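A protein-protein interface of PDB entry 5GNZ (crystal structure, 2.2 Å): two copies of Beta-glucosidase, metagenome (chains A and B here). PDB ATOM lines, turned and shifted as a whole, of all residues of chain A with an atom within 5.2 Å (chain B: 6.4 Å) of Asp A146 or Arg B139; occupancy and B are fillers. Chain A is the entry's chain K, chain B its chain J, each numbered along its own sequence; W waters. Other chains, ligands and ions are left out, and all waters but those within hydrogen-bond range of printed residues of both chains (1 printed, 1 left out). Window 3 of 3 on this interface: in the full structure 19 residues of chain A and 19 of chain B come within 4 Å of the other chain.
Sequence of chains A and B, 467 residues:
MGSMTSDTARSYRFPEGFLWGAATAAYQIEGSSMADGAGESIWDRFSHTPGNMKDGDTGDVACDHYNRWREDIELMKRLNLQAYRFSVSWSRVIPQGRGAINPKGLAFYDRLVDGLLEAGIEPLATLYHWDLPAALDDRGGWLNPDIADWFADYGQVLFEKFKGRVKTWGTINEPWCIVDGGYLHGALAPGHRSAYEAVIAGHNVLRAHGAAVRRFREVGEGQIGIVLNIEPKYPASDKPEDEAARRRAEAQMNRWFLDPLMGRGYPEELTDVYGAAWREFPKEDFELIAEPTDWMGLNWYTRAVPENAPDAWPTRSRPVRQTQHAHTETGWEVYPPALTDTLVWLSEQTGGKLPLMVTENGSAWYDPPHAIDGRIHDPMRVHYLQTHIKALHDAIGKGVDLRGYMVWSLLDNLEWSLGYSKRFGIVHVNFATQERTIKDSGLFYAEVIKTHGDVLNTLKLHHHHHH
O of Arg B139 is in hydrogen-bond range of ND2 of Asn B144 (2.9 Å). The side-chain amide nitrogen (ND2) of Asn A144 lies within hydrogen-bond range of the backbone carbonyl oxygen (O) of Arg A139 (2.9 Å). N of Asp A146 sits at hydrogen-bond distance from OD1 of Asn A144.
Water W1 bridges O of Leu B143 (2.9 Å) and OD2 of Asp A138 (3.3 Å).
Arg B139 touches Asp A138. Asp A138 touches Gly B140 (O to CA, 3.4 Å). Leu B143 touches Asp A138 (C to O, 3.5 Å). O of Arg A139 touches O of Asp B138, 3.9 Å away. Gly B140 touches Arg A139 (N to C, 3.6 Å). Asp B138 touches Gly A140 (O to CA, 3.5 Å). N of Gly A140 touches C of Arg B139 (3.7 Å). N of Gly A140 touches CA of Gly B140, 3.4 Å away.
Asp A138 touches Arg B139, and with the chains exchanged Arg A139 touches Asp B138. Asp A138 touches Gly B140, and with the chains exchanged Gly A140 touches Asp B138. Arg B139 touches its own counterpart, Arg A139. Arg A139 touches Gly B140, and with the chains exchanged Gly A140 touches Arg B139. Positions printed for both chains: 138, 139, 140, 144 and 150.
N of Asn A144 lies within hydrogen-bond range of O of Asp B138 (3.3 Å). The guanidinium group of Arg B139 sits at hydrogen-bond distance from the side-chain amide oxygen of Asn A144, at 2.9 Å. OD2 of Asp A146 is in salt-bridge range of NH1 of Arg B139 (2.9 Å). N of Asn B144 lies within hydrogen-bond range of O of Asp A138 (3.4 Å). The side-chain amide oxygen (OD1) of Asn B144 is in hydrogen-bond range of the guanidinium group (NH1) of Arg A139, 3.1 Å away. The backbone carbonyl oxygen (O) of Arg A139 sits close to the backbone carbonyl oxygen (O) of Arg B139.
Hydrophobic or aromatic side chains of chain B within 4 Å of the printed part of chain A: Leu B143. Along chain B the printed residues that touch a printed residue of chain A span positions 138 to 144. Of the 11 printed residues of chain A, 5 touch a printed residue of chain B. Printed residues of chain A that touch a printed residue of chain B: Asp A138, Arg A139, Gly A140, Asn A144 and Asp A146. Among the printed residues, Asp or Glu carboxylates within 4 Å of a Lys or Arg side-chain nitrogen of the other chain: Asp A146 with Arg B139.
Asp A146 touches just one residue of chain B: Arg B139. Printed residues of chain A within 4 Å of Arg B139: Asp A138 (3.9 Å), Arg A139 (3.1 Å), Gly A140 (3.7 Å), Asn A144 (2.9 Å) and Asp A146 (2.9 Å). Of the printed residues of chain A, Asn B144 touches Asp A138 (3.4 Å) and Arg A139 (3.1 Å). Of the printed residues of chain A, Leu B143 touches Asp A138. Printed residues of chain B within 4 Å of Gly A140: Asp B138, Arg B139 and Gly B140. The nearest printed residue of chain B that does not touch Asp A146 is Asp B138 (7.4 Å). The nearest printed residue of chain A that does not touch Arg B139 is Pro A145 (4.01 Å).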
ATOM      1  N   ASP A 138      -2.675 -22.000   8.426  1.00  0.00           N
ATOM      2  CA  ASP A 138      -2.437 -20.563   8.433  1.00  0.00           C
ATOM      3  C   ASP A 138      -3.493 -19.837   7.600  1.00  0.00           C
ATOM      4  O   ASP A 138      -3.640 -18.617   7.696  1.00  0.00           O
ATOM      5  CB  ASP A 138      -1.031 -20.242   7.918  1.00  0.00           C
ATOM      6  CG  ASP A 138       0.061 -20.723   8.858  1.00  0.00           C
ATOM      7  OD1 ASP A 138      -0.238 -20.964  10.044  1.00  0.00           O
ATOM      8  OD2 ASP A 138       1.220 -20.850   8.408  1.00  0.00           O
ATOM      9  N   ARG A 139      -4.226 -20.588   6.784  1.00  0.00           N
ATOM     10  CA  ARG A 139      -5.349 -20.025   6.041  1.00  0.00           C
ATOM     11  C   ARG A 139      -6.679 -20.371   6.707  1.00  0.00           C
ATOM     12  O   ARG A 139      -7.740 -20.200   6.109  1.00  0.00           O
ATOM     13  CB  ARG A 139      -5.345 -20.528   4.592  1.00  0.00           C
ATOM     14  CG  ARG A 139      -4.003 -20.415   3.899  1.00  0.00           C
ATOM     15  CD  ARG A 139      -3.676 -18.981   3.535  1.00  0.00           C
ATOM     16  NE  ARG A 139      -2.443 -18.888   2.760  1.00  0.00           N
ATOM     17  CZ  ARG A 139      -2.118 -17.857   1.989  1.00  0.00           C
ATOM     18  NH1 ARG A 139      -2.935 -16.818   1.891  1.00  0.00           N
ATOM     19  NH2 ARG A 139      -0.974 -17.862   1.321  1.00  0.00           N
ATOM     20  N   GLY A 140      -6.618 -20.857   7.942  1.00  0.00           N
ATOM     21  CA  GLY A 140      -7.818 -21.091   8.724  1.00  0.00           C
ATOM     22  C   GLY A 140      -8.141 -22.560   8.905  1.00  0.00           C
ATOM     23  O   GLY A 140      -8.985 -22.923   9.727  1.00  0.00           O
ATOM     24  N   ASN A 144     -11.919 -22.692   7.305  1.00  0.00           N
ATOM     25  CA  ASN A 144     -12.053 -22.053   6.002  1.00  0.00           C
ATOM     26  C   ASN A 144     -12.813 -22.977   5.064  1.00  0.00           C
ATOM     27  O   ASN A 144     -12.330 -24.057   4.742  1.00  0.00           O
ATOM     28  CB  ASN A 144     -10.672 -21.714   5.429  1.00  0.00           C
ATOM     29  CG  ASN A 144     -10.740 -20.827   4.192  1.00  0.00           C
ATOM     30  OD1 ASN A 144     -11.679 -20.898   3.400  1.00  0.00           O
ATOM     31  ND2 ASN A 144      -9.723 -19.992   4.018  1.00  0.00           N
ATOM     32  N   PRO A 145     -14.004 -22.549   4.617  1.00  0.00           N
ATOM     33  CA  PRO A 145     -14.852 -23.363   3.737  1.00  0.00           C
ATOM     34  C   PRO A 145     -14.145 -23.769   2.447  1.00  0.00           C
ATOM     35  O   PRO A 145     -14.432 -24.843   1.896  1.00  0.00           O
ATOM     36  CB  PRO A 145     -16.039 -22.436   3.436  1.00  0.00           C
ATOM     37  CG  PRO A 145     -15.555 -21.055   3.759  1.00  0.00           C
ATOM     38  CD  PRO A 145     -14.604 -21.236   4.899  1.00  0.00           C
ATOM     39  N   ASP A 146     -13.186 -22.954   2.011  1.00  0.00           N
ATOM     40  CA  ASP A 146     -12.440 -23.231   0.790  1.00  0.00           C
ATOM     41  C   ASP A 146     -11.702 -24.562   0.873  1.00  0.00           C
ATOM     42  O   ASP A 146     -11.294 -25.114  -0.148  1.00  0.00           O
ATOM     43  CB  ASP A 146     -11.429 -22.115   0.506  1.00  0.00           C
ATOM     44  CG  ASP A 146     -12.087 -20.787   0.193  1.00  0.00           C
ATOM     45  OD1 ASP A 146     -13.319 -20.758   0.009  1.00  0.00           O
ATOM     46  OD2 ASP A 146     -11.361 -19.770   0.124  1.00  0.00           O
ATOM     47  N   ILE A 147     -11.547 -25.086   2.087  1.00  0.00           N
ATOM     48  CA  ILE A 147     -10.841 -26.345   2.270  1.00  0.00           C
ATOM     49  C   ILE A 147     -11.552 -27.471   1.539  1.00  0.00           C
ATOM     50  O   ILE A 147     -10.902 -28.412   1.074  1.00  0.00           O
ATOM     51  CB  ILE A 147     -10.682 -26.715   3.763  1.00  0.00           C
ATOM     52  CG1 ILE A 147      -9.656 -27.837   3.920  1.00  0.00           C
ATOM     53  CG2 ILE A 147     -12.017 -27.111   4.391  1.00  0.00           C
ATOM     54  CD1 ILE A 147      -9.083 -27.954   5.305  1.00  0.00           C
ATOM     55  N   ALA A 148     -12.872 -27.345   1.379  1.00  0.00           N
ATOM     56  CA  ALA A 148     -13.630 -28.367   0.668  1.00  0.00           C
ATOM     57  C   ALA A 148     -13.042 -28.528  -0.724  1.00  0.00           C
ATOM     58  O   ALA A 148     -12.905 -29.641  -1.234  1.00  0.00           O
ATOM     59  CB  ALA A 148     -15.104 -28.003   0.600  1.00  0.00           C
ATOM     60  N   ASP A 149     -12.681 -27.402  -1.330  1.00  0.00           N
ATOM     61  CA  ASP A 149     -12.046 -27.421  -2.631  1.00  0.00           C
ATOM     62  C   ASP A 149     -10.605 -27.921  -2.532  1.00  0.00           C
ATOM     63  O   ASP A 149     -10.196 -28.778  -3.323  1.00  0.00           O
ATOM     64  CB  ASP A 149     -12.100 -26.027  -3.252  1.00  0.00           C
ATOM     65  CG  ASP A 149     -13.520 -25.557  -3.489  1.00  0.00           C
ATOM     66  OD1 ASP A 149     -14.369 -26.400  -3.846  1.00  0.00           O
ATOM     67  OD2 ASP A 149     -13.786 -24.350  -3.309  1.00  0.00           O
ATOM     68  N   TRP A 150      -9.864 -27.445  -1.528  1.00  0.00           N
ATOM     69  CA  TRP A 150      -8.450 -27.798  -1.404  1.00  0.00           C
ATOM     70  C   TRP A 150      -8.332 -29.302  -1.316  1.00  0.00           C
ATOM     71  O   TRP A 150      -7.608 -29.936  -2.089  1.00  0.00           O
ATOM     72  CB  TRP A 150      -7.809 -27.169  -0.163  1.00  0.00           C
ATOM     73  CG  TRP A 150      -7.862 -25.676  -0.084  1.00  0.00           C
ATOM     74  CD1 TRP A 150      -8.022 -24.802  -1.115  1.00  0.00           C
ATOM     75  CD2 TRP A 150      -7.749 -24.880   1.106  1.00  0.00           C
ATOM     76  NE1 TRP A 150      -8.017 -23.510  -0.645  1.00  0.00           N
ATOM     77  CE2 TRP A 150      -7.849 -23.532   0.714  1.00  0.00           C
ATOM     78  CE3 TRP A 150      -7.571 -25.177   2.459  1.00  0.00           C
ATOM     79  CZ2 TRP A 150      -7.779 -22.483   1.634  1.00  0.00           C
ATOM     80  CZ3 TRP A 150      -7.503 -24.135   3.369  1.00  0.00           C
ATOM     81  CH2 TRP A 150      -7.605 -22.807   2.952  1.00  0.00           C
ATOM     82  N   ARG A 207     -18.359 -31.171   4.461  1.00  0.00           N
ATOM     83  CA  ARG A 207     -18.341 -30.616   3.111  1.00  0.00           C
ATOM     84  C   ARG A 207     -17.132 -31.100   2.314  1.00  0.00           C
ATOM     85  O   ARG A 207     -17.249 -31.388   1.120  1.00  0.00           O
ATOM     86  CB  ARG A 207     -18.349 -29.088   3.152  1.00  0.00           C
ATOM     87  CG  ARG A 207     -19.689 -28.467   3.517  1.00  0.00           C
ATOM     88  CD  ARG A 207     -19.623 -26.946   3.469  1.00  0.00           C
ATOM     89  NE  ARG A 207     -19.198 -26.451   2.160  1.00  0.00           N
ATOM     90  CZ  ARG A 207     -17.997 -25.940   1.905  1.00  0.00           C
ATOM     91  NH1 ARG A 207     -17.095 -25.851   2.869  1.00  0.00           N
ATOM     92  NH2 ARG A 207     -17.696 -25.521   0.686  1.00  0.00           N
ATOM     93  N   ALA B 134     -14.504 -12.342  13.259  1.00  0.00           N
ATOM     94  CA  ALA B 134     -14.387 -13.794  13.334  1.00  0.00           C
ATOM     95  C   ALA B 134     -14.307 -14.442  11.957  1.00  0.00           C
ATOM     96  O   ALA B 134     -13.689 -15.497  11.792  1.00  0.00           O
ATOM     97  CB  ALA B 134     -15.556 -14.371  14.116  1.00  0.00           C
ATOM     98  N   ALA B 135     -14.943 -13.812  10.974  1.00  0.00           N
ATOM     99  CA  ALA B 135     -14.933 -14.317   9.609  1.00  0.00           C
ATOM    100  C   ALA B 135     -13.531 -14.316   9.011  1.00  0.00           C
ATOM    101  O   ALA B 135     -13.203 -15.162   8.183  1.00  0.00           O
ATOM    102  CB  ALA B 135     -15.871 -13.495   8.744  1.00  0.00           C
ATOM    103  N   LEU B 136     -12.711 -13.354   9.423  1.00  0.00           N
ATOM    104  CA  LEU B 136     -11.328 -13.281   8.962  1.00  0.00           C
ATOM    105  C   LEU B 136     -10.437 -14.231   9.750  1.00  0.00           C
ATOM    106  O   LEU B 136      -9.445 -14.739   9.229  1.00  0.00           O
ATOM    107  CB  LEU B 136     -10.796 -11.851   9.063  1.00  0.00           C
ATOM    108  CG  LEU B 136     -11.506 -10.822   8.184  1.00  0.00           C
ATOM    109  CD1 LEU B 136     -10.790  -9.488   8.233  1.00  0.00           C
ATOM    110  CD2 LEU B 136     -11.596 -11.330   6.756  1.00  0.00           C
ATOM    111  N   ASP B 137     -10.792 -14.458  11.010  1.00  0.00           N
ATOM    112  CA  ASP B 137     -10.099 -15.443  11.826  1.00  0.00           C
ATOM    113  C   ASP B 137     -10.308 -16.838  11.258  1.00  0.00           C
ATOM    114  O   ASP B 137      -9.420 -17.689  11.333  1.00  0.00           O
ATOM    115  CB  ASP B 137     -10.583 -15.385  13.273  1.00  0.00           C
ATOM    116  CG  ASP B 137      -9.607 -16.032  14.240  1.00  0.00           C
ATOM    117  OD1 ASP B 137      -8.423 -15.637  14.234  1.00  0.00           O
ATOM    118  OD2 ASP B 137     -10.021 -16.928  15.005  1.00  0.00           O
ATOM    119  N   ASP B 138     -11.487 -17.061  10.682  1.00  0.00           N
ATOM    120  CA  ASP B 138     -11.796 -18.331  10.034  1.00  0.00           C
ATOM    121  C   ASP B 138     -10.998 -18.518   8.744  1.00  0.00           C
ATOM    122  O   ASP B 138     -10.923 -19.624   8.207  1.00  0.00           O
ATOM    123  CB  ASP B 138     -13.298 -18.424   9.743  1.00  0.00           C
ATOM    124  CG  ASP B 138     -14.133 -18.493  11.009  1.00  0.00           C
ATOM    125  OD1 ASP B 138     -13.576 -18.836  12.072  1.00  0.00           O
ATOM    126  OD2 ASP B 138     -15.346 -18.201  10.938  1.00  0.00           O
ATOM    127  N   ARG B 139     -10.412 -17.434   8.247  1.00  0.00           N
ATOM    128  CA  ARG B 139      -9.517 -17.506   7.096  1.00  0.00           C
ATOM    129  C   ARG B 139      -8.053 -17.469   7.527  1.00  0.00           C
ATOM    130  O   ARG B 139      -7.163 -17.261   6.702  1.00  0.00           O
ATOM    131  CB  ARG B 139      -9.797 -16.360   6.115  1.00  0.00           C
ATOM    132  CG  ARG B 139     -11.255 -16.193   5.697  1.00  0.00           C
ATOM    133  CD  ARG B 139     -11.667 -17.267   4.703  1.00  0.00           C
ATOM    134  NE  ARG B 139     -13.008 -17.045   4.169  1.00  0.00           N
ATOM    135  CZ  ARG B 139     -13.453 -17.567   3.030  1.00  0.00           C
ATOM    136  NH1 ARG B 139     -12.668 -18.348   2.305  1.00  0.00           N
ATOM    137  NH2 ARG B 139     -14.684 -17.310   2.615  1.00  0.00           N
ATOM    138  N   GLY B 140      -7.807 -17.676   8.818  1.00  0.00           N
ATOM    139  CA  GLY B 140      -6.452 -17.794   9.332  1.00  0.00           C
ATOM    140  C   GLY B 140      -6.010 -16.617  10.183  1.00  0.00           C
ATOM    141  O   GLY B 140      -4.982 -16.681  10.860  1.00  0.00           O
ATOM    142  N   GLY B 141      -6.799 -15.549  10.166  1.00  0.00           N
ATOM    143  CA  GLY B 141      -6.484 -14.354  10.929  1.00  0.00           C
ATOM    144  C   GLY B 141      -5.117 -13.768  10.630  1.00  0.00           C
ATOM    145  O   GLY B 141      -4.751 -13.585   9.469  1.00  0.00           O
ATOM    146  N   LEU B 143      -2.384 -15.083  10.782  1.00  0.00           N
ATOM    147  CA  LEU B 143      -1.491 -16.072  10.186  1.00  0.00           C
ATOM    148  C   LEU B 143      -1.574 -16.025   8.666  1.00  0.00           C
ATOM    149  O   LEU B 143      -0.715 -16.565   7.973  1.00  0.00           O
ATOM    150  CB  LEU B 143      -1.836 -17.475  10.690  1.00  0.00           C
ATOM    151  CG  LEU B 143      -1.825 -17.653  12.211  1.00  0.00           C
ATOM    152  CD1 LEU B 143      -2.233 -19.062  12.600  1.00  0.00           C
ATOM    153  CD2 LEU B 143      -0.460 -17.310  12.795  1.00  0.00           C
ATOM    154  N   ASN B 144      -2.617 -15.381   8.153  1.00  0.00           N
ATOM    155  CA  ASN B 144      -2.810 -15.237   6.713  1.00  0.00           C
ATOM    156  C   ASN B 144      -2.249 -13.905   6.228  1.00  0.00           C
ATOM    157  O   ASN B 144      -2.745 -12.851   6.612  1.00  0.00           O
ATOM    158  CB  ASN B 144      -4.298 -15.354   6.371  1.00  0.00           C
ATOM    159  CG  ASN B 144      -4.562 -15.438   4.875  1.00  0.00           C
ATOM    160  OD1 ASN B 144      -3.841 -14.863   4.061  1.00  0.00           O
ATOM    161  ND2 ASN B 144      -5.620 -16.148   4.510  1.00  0.00           N
ATOM    162  N   TRP B 150      -6.426  -6.937   3.648  1.00  0.00           N
ATOM    163  CA  TRP B 150      -7.767  -6.812   4.215  1.00  0.00           C
ATOM    164  C   TRP B 150      -7.793  -5.584   5.094  1.00  0.00           C
ATOM    165  O   TRP B 150      -8.634  -4.695   4.927  1.00  0.00           O
ATOM    166  CB  TRP B 150      -8.165  -8.049   5.033  1.00  0.00           C
ATOM    167  CG  TRP B 150      -8.147  -9.344   4.281  1.00  0.00           C
ATOM    168  CD1 TRP B 150      -8.225  -9.507   2.930  1.00  0.00           C
ATOM    169  CD2 TRP B 150      -8.054 -10.663   4.840  1.00  0.00           C
ATOM    170  NE1 TRP B 150      -8.180 -10.842   2.612  1.00  0.00           N
ATOM    171  CE2 TRP B 150      -8.075 -11.574   3.767  1.00  0.00           C
ATOM    172  CE3 TRP B 150      -7.951 -11.162   6.142  1.00  0.00           C
ATOM    173  CZ2 TRP B 150      -7.997 -12.955   3.956  1.00  0.00           C
ATOM    174  CZ3 TRP B 150      -7.871 -12.534   6.326  1.00  0.00           C
ATOM    175  CH2 TRP B 150      -7.893 -13.411   5.242  1.00  0.00           C
HETATM  176  O   HOH W   1       1.274 -18.120   6.540  1.00  0.00           O
